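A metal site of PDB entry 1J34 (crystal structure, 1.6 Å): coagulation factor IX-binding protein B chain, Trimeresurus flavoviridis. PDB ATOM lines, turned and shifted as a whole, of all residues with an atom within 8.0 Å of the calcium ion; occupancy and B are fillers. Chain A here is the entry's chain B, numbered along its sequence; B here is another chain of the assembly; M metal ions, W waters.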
ATOM      1  N   TYR A   9     -11.688  14.621  -6.711  1.00  0.00           N
ATOM      2  CA  TYR A   9     -11.405  13.445  -7.525  1.00  0.00           C
ATOM      3  C   TYR A   9     -10.683  13.886  -8.790  1.00  0.00           C
ATOM      4  O   TYR A   9     -11.200  14.704  -9.564  1.00  0.00           O
ATOM      5  CB  TYR A   9     -12.671  12.687  -7.932  1.00  0.00           C
ATOM      6  CG  TYR A   9     -12.386  11.528  -8.871  1.00  0.00           C
ATOM      7  CD1 TYR A   9     -11.847  10.328  -8.408  1.00  0.00           C
ATOM      8  CD2 TYR A   9     -12.588  11.667 -10.250  1.00  0.00           C
ATOM      9  CE1 TYR A   9     -11.500   9.300  -9.282  1.00  0.00           C
ATOM     10  CE2 TYR A   9     -12.243  10.644 -11.137  1.00  0.00           C
ATOM     11  CZ  TYR A   9     -11.695   9.466 -10.650  1.00  0.00           C
ATOM     12  OH  TYR A   9     -11.326   8.477 -11.525  1.00  0.00           O
ATOM     13  N   HIS A  12     -10.671  17.563  -9.918  1.00  0.00           N
ATOM     14  CA  HIS A  12     -11.958  18.241  -9.997  1.00  0.00           C
ATOM     15  C   HIS A  12     -12.699  18.168  -8.666  1.00  0.00           C
ATOM     16  O   HIS A  12     -12.360  17.361  -7.801  1.00  0.00           O
ATOM     17  CB  HIS A  12     -12.833  17.643 -11.115  1.00  0.00           C
ATOM     18  CG  HIS A  12     -12.416  18.058 -12.491  1.00  0.00           C
ATOM     19  ND1 HIS A  12     -13.114  17.694 -13.627  1.00  0.00           N
ATOM     20  CD2 HIS A  12     -11.388  18.826 -12.929  1.00  0.00           C
ATOM     21  CE1 HIS A  12     -12.538  18.218 -14.688  1.00  0.00           C
ATOM     22  NE2 HIS A  12     -11.487  18.907 -14.297  1.00  0.00           N
ATOM     23  N   CYS A  13     -13.709  19.019  -8.513  1.00  0.00           N
ATOM     24  CA  CYS A  13     -14.510  19.054  -7.293  1.00  0.00           C
ATOM     25  C   CYS A  13     -15.960  18.737  -7.616  1.00  0.00           C
ATOM     26  O   CYS A  13     -16.518  19.265  -8.579  1.00  0.00           O
ATOM     27  CB  CYS A  13     -14.415  20.437  -6.643  1.00  0.00           C
ATOM     28  SG  CYS A  13     -12.721  20.902  -6.179  1.00  0.00           S
ATOM     29  N   TYR A  14     -16.566  17.874  -6.806  1.00  0.00           N
ATOM     30  CA  TYR A  14     -17.951  17.446  -6.998  1.00  0.00           C
ATOM     31  C   TYR A  14     -18.781  17.613  -5.734  1.00  0.00           C
ATOM     32  O   TYR A  14     -18.267  17.484  -4.620  1.00  0.00           O
ATOM     33  CB  TYR A  14     -17.986  15.963  -7.410  1.00  0.00           C
ATOM     34  CG  TYR A  14     -17.105  15.621  -8.584  1.00  0.00           C
ATOM     35  CD1 TYR A  14     -15.728  15.491  -8.428  1.00  0.00           C
ATOM     36  CD2 TYR A  14     -17.643  15.424  -9.850  1.00  0.00           C
ATOM     37  CE1 TYR A  14     -14.905  15.169  -9.518  1.00  0.00           C
ATOM     38  CE2 TYR A  14     -16.848  15.113 -10.940  1.00  0.00           C
ATOM     39  CZ  TYR A  14     -15.475  14.991 -10.773  1.00  0.00           C
ATOM     40  OH  TYR A  14     -14.678  14.669 -11.837  1.00  0.00           O
ATOM     41  N   LEU A  39     -23.336  21.120 -14.203  1.00  0.00           N
ATOM     42  CA  LEU A  39     -23.841  19.817 -13.797  1.00  0.00           C
ATOM     43  C   LEU A  39     -22.686  18.885 -14.131  1.00  0.00           C
ATOM     44  O   LEU A  39     -21.930  19.150 -15.072  1.00  0.00           O
ATOM     45  CB  LEU A  39     -25.087  19.428 -14.597  1.00  0.00           C
ATOM     46  CG  LEU A  39     -26.401  19.988 -14.067  1.00  0.00           C
ATOM     47  CD1 LEU A  39     -27.519  19.686 -15.058  1.00  0.00           C
ATOM     48  CD2 LEU A  39     -26.716  19.365 -12.711  1.00  0.00           C
ATOM     49  N   VAL A  40     -22.539  17.808 -13.369  1.00  0.00           N
ATOM     50  CA  VAL A  40     -21.453  16.866 -13.568  1.00  0.00           C
ATOM     51  C   VAL A  40     -21.394  16.234 -14.962  1.00  0.00           C
ATOM     52  O   VAL A  40     -22.422  15.917 -15.560  1.00  0.00           O
ATOM     53  CB  VAL A  40     -21.507  15.742 -12.506  1.00  0.00           C
ATOM     54  CG1 VAL A  40     -22.768  14.905 -12.700  1.00  0.00           C
ATOM     55  CG2 VAL A  40     -20.245  14.900 -12.572  1.00  0.00           C
ATOM     56  N   SER A  41     -20.177  16.075 -15.466  1.00  0.00           N
ATOM     57  CA  SER A  41     -19.945  15.460 -16.770  1.00  0.00           C
ATOM     58  C   SER A  41     -19.046  14.245 -16.566  1.00  0.00           C
ATOM     59  O   SER A  41     -18.110  14.301 -15.762  1.00  0.00           O
ATOM     60  CB  SER A  41     -19.276  16.454 -17.717  1.00  0.00           C
ATOM     61  OG  SER A  41     -18.011  16.865 -17.218  1.00  0.00           O
ATOM     62  N   PHE A  42     -19.323  13.159 -17.263  1.00  0.00           N
ATOM     63  CA  PHE A  42     -18.500  11.959 -17.130  1.00  0.00           C
ATOM     64  C   PHE A  42     -17.615  11.758 -18.352  1.00  0.00           C
ATOM     65  O   PHE A  42     -18.102  11.465 -19.448  1.00  0.00           O
ATOM     66  CB  PHE A  42     -19.378  10.709 -16.920  1.00  0.00           C
ATOM     67  CG  PHE A  42     -20.192  10.737 -15.655  1.00  0.00           C
ATOM     68  CD1 PHE A  42     -19.749  11.437 -14.528  1.00  0.00           C
ATOM     69  CD2 PHE A  42     -21.398  10.046 -15.584  1.00  0.00           C
ATOM     70  CE1 PHE A  42     -20.484  11.424 -13.351  1.00  0.00           C
ATOM     71  CE2 PHE A  42     -22.136  10.024 -14.402  1.00  0.00           C
ATOM     72  CZ  PHE A  42     -21.687  10.725 -13.291  1.00  0.00           C
ATOM     73  N   GLN A  43     -16.315  11.909 -18.154  1.00  0.00           N
ATOM     74  CA  GLN A  43     -15.340  11.738 -19.233  1.00  0.00           C
ATOM     75  C   GLN A  43     -14.735  10.336 -19.188  1.00  0.00           C
ATOM     76  O   GLN A  43     -13.968   9.963 -20.078  1.00  0.00           O
ATOM     77  CB  GLN A  43     -14.224  12.784 -19.113  1.00  0.00           C
ATOM     78  CG  GLN A  43     -14.594  14.213 -19.541  1.00  0.00           C
ATOM     79  CD  GLN A  43     -15.756  14.812 -18.739  1.00  0.00           C
ATOM     80  OE1 GLN A  43     -15.865  14.593 -17.533  1.00  0.00           O
ATOM     81  NE2 GLN A  43     -16.606  15.576 -19.411  1.00  0.00           N
ATOM     82  N   SER A  44     -15.085   9.575 -18.158  1.00  0.00           N
ATOM     83  CA  SER A  44     -14.576   8.208 -18.026  1.00  0.00           C
ATOM     84  C   SER A  44     -15.398   7.432 -17.010  1.00  0.00           C
ATOM     85  O   SER A  44     -16.123   8.015 -16.212  1.00  0.00           O
ATOM     86  CB  SER A  44     -13.109   8.226 -17.576  1.00  0.00           C
ATOM     87  OG  SER A  44     -12.988   8.712 -16.254  1.00  0.00           O
ATOM     88  N   GLU A  47     -14.426   8.148 -13.290  1.00  0.00           N
ATOM     89  CA  GLU A  47     -15.036   9.373 -12.777  1.00  0.00           C
ATOM     90  C   GLU A  47     -16.490   9.102 -12.417  1.00  0.00           C
ATOM     91  O   GLU A  47     -16.956   9.498 -11.354  1.00  0.00           O
ATOM     92  CB  GLU A  47     -14.943  10.491 -13.823  1.00  0.00           C
ATOM     93  CG  GLU A  47     -15.654  11.765 -13.403  1.00  0.00           C
ATOM     94  CD  GLU A  47     -15.538  12.870 -14.433  1.00  0.00           C
ATOM     95  OE1 GLU A  47     -15.235  12.573 -15.608  1.00  0.00           O
ATOM     96  OE2 GLU A  47     -15.771  14.046 -14.071  1.00  0.00           O
ATOM     97  N   ALA A  48     -17.204   8.419 -13.310  1.00  0.00           N
ATOM     98  CA  ALA A  48     -18.607   8.116 -13.061  1.00  0.00           C
ATOM     99  C   ALA A  48     -18.760   7.301 -11.788  1.00  0.00           C
ATOM    100  O   ALA A  48     -19.657   7.560 -10.980  1.00  0.00           O
ATOM    101  CB  ALA A  48     -19.192   7.347 -14.242  1.00  0.00           C
ATOM    102  N   VAL A  51     -18.462   9.592  -8.712  1.00  0.00           N
ATOM    103  CA  VAL A  51     -19.645  10.418  -8.529  1.00  0.00           C
ATOM    104  C   VAL A  51     -20.874   9.648  -8.041  1.00  0.00           C
ATOM    105  O   VAL A  51     -21.570  10.089  -7.129  1.00  0.00           O
ATOM    106  CB  VAL A  51     -19.998  11.165  -9.827  1.00  0.00           C
ATOM    107  CG1 VAL A  51     -21.282  11.977  -9.633  1.00  0.00           C
ATOM    108  CG2 VAL A  51     -18.850  12.092 -10.217  1.00  0.00           C
ATOM    109  N   GLU A 120     -20.106  20.097 -10.596  1.00  0.00           N
ATOM    110  CA  GLU A 120     -18.682  19.839 -10.753  1.00  0.00           C
ATOM    111  C   GLU A 120     -17.955  21.062 -11.323  1.00  0.00           C
ATOM    112  O   GLU A 120     -18.542  21.849 -12.072  1.00  0.00           O
ATOM    113  CB  GLU A 120     -18.458  18.647 -11.708  1.00  0.00           C
ATOM    114  CG  GLU A 120     -17.039  18.555 -12.296  1.00  0.00           C
ATOM    115  CD  GLU A 120     -16.884  17.481 -13.370  1.00  0.00           C
ATOM    116  OE1 GLU A 120     -17.890  17.134 -14.029  1.00  0.00           O
ATOM    117  OE2 GLU A 120     -15.753  16.998 -13.579  1.00  0.00           O
ATOM    118  N   PHE A 121     -16.696  21.226 -10.952  1.00  0.00           N
ATOM    119  CA  PHE A 121     -15.880  22.312 -11.488  1.00  0.00           C
ATOM    120  C   PHE A 121     -14.427  21.886 -11.381  1.00  0.00           C
ATOM    121  O   PHE A 121     -14.093  20.981 -10.610  1.00  0.00           O
ATOM    122  CB  PHE A 121     -16.143  23.640 -10.735  1.00  0.00           C
ATOM    123  CG  PHE A 121     -15.595  23.690  -9.332  1.00  0.00           C
ATOM    124  CD1 PHE A 121     -14.241  23.890  -9.094  1.00  0.00           C
ATOM    125  CD2 PHE A 121     -16.451  23.542  -8.245  1.00  0.00           C
ATOM    126  CE1 PHE A 121     -13.738  23.947  -7.800  1.00  0.00           C
ATOM    127  CE2 PHE A 121     -15.968  23.601  -6.941  1.00  0.00           C
ATOM    128  CZ  PHE A 121     -14.602  23.804  -6.711  1.00  0.00           C
ATOM    129  N   TRP B  83     -21.126  18.343 -23.459  1.00  0.00           N
ATOM    130  CA  TRP B  83     -21.605  18.513 -22.090  1.00  0.00           C
ATOM    131  C   TRP B  83     -21.844  19.994 -21.837  1.00  0.00           C
ATOM    132  O   TRP B  83     -21.369  20.835 -22.605  1.00  0.00           O
ATOM    133  CB  TRP B  83     -20.574  18.006 -21.080  1.00  0.00           C
ATOM    134  CG  TRP B  83     -20.315  16.540 -21.159  1.00  0.00           C
ATOM    135  CD1 TRP B  83     -19.339  15.909 -21.886  1.00  0.00           C
ATOM    136  CD2 TRP B  83     -21.025  15.506 -20.472  1.00  0.00           C
ATOM    137  NE1 TRP B  83     -19.404  14.552 -21.686  1.00  0.00           N
ATOM    138  CE2 TRP B  83     -20.427  14.282 -20.813  1.00  0.00           C
ATOM    139  CE3 TRP B  83     -22.114  15.511 -19.583  1.00  0.00           C
ATOM    140  CZ2 TRP B  83     -20.876  13.059 -20.310  1.00  0.00           C
ATOM    141  CZ3 TRP B  83     -22.563  14.287 -19.080  1.00  0.00           C
ATOM    142  CH2 TRP B  83     -21.943  13.076 -19.449  1.00  0.00           C
ATOM    143  N   ASP B  85     -20.480  21.764 -19.797  1.00  0.00           N
ATOM    144  CA  ASP B  85     -19.220  22.425 -19.485  1.00  0.00           C
ATOM    145  C   ASP B  85     -18.383  22.682 -20.739  1.00  0.00           C
ATOM    146  O   ASP B  85     -17.234  23.112 -20.645  1.00  0.00           O
ATOM    147  CB  ASP B  85     -18.399  21.626 -18.455  1.00  0.00           C
ATOM    148  CG  ASP B  85     -17.914  20.281 -18.991  1.00  0.00           C
ATOM    149  OD1 ASP B  85     -17.989  20.024 -20.212  1.00  0.00           O
ATOM    150  OD2 ASP B  85     -17.418  19.477 -18.163  1.00  0.00           O
ATOM    151  N   SER B  87     -17.133  20.550 -22.912  1.00  0.00           N
ATOM    152  CA  SER B  87     -16.318  19.431 -23.392  1.00  0.00           C
ATOM    153  C   SER B  87     -17.113  18.455 -24.239  1.00  0.00           C
ATOM    154  O   SER B  87     -18.325  18.299 -24.070  1.00  0.00           O
ATOM    155  CB  SER B  87     -15.675  18.696 -22.217  1.00  0.00           C
ATOM    156  OG  SER B  87     -16.635  18.054 -21.408  1.00  0.00           O
HETATM  157 CA    CA M   1     -16.241  15.769 -15.629  1.00  0.00          CA
HETATM  158  O   HOH W   1     -15.440  17.933 -16.337  1.00  0.00           O
HETATM  159  O   HOH W   2     -13.768  15.439 -15.627  1.00  0.00           O
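The side-chain amide nitrogen (NE2) of Gln 43 sits at hydrogen-bond distance from the side-chain hydroxyl (OG) of Ser 87 of chain B (3.2 Å). The side-chain carboxylate of Glu 120 sits close to the side-chain hydroxyl of Tyr 14, 3.1 Å away. N of Glu 47 lies within hydrogen-bond range of OG of Ser 44, at 3.3 Å. The side-chain carboxylate (OE2) of Glu 120 lies close to a ring nitrogen (ND1) of His 12 (2.7 Å). The side-chain carboxylate (OE2) of Glu 47 lies close to the side-chain hydroxyl (OH) of Tyr 14, at 2.6 Å. The side-chain hydroxyl (OG) of Ser 41 lies close to the side-chain carboxylate (OD2) of Asp 85 of chain B (2.8 Å).
Four residues have an atom within 4 Å of the calcium ion: Ser 41, Gln 43, Glu 47 and Glu 120.
The calcium ion is bound by OE1 of Gln 43 (2.3 Å). The side-chain carboxylate (OE2) of Glu 47 is bound to the calcium ion (2.4 Å). O of Ser 41 binds the calcium ion (2.4 Å). Water W1 is bound to the calcium ion, at 2.4 Å. OE2 of Glu 120 binds the calcium ion. The calcium ion is bound by water W2, at 2.5 Å. The calcium ion is bound by OG of Ser 41. OE1 of Glu 120 is bound to the calcium ion (2.7 Å).
Water W2 lies within hydrogen-bond range of ND1 of His 12 (3.1 Å) and OE1 of Glu 47 (3.2 Å).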
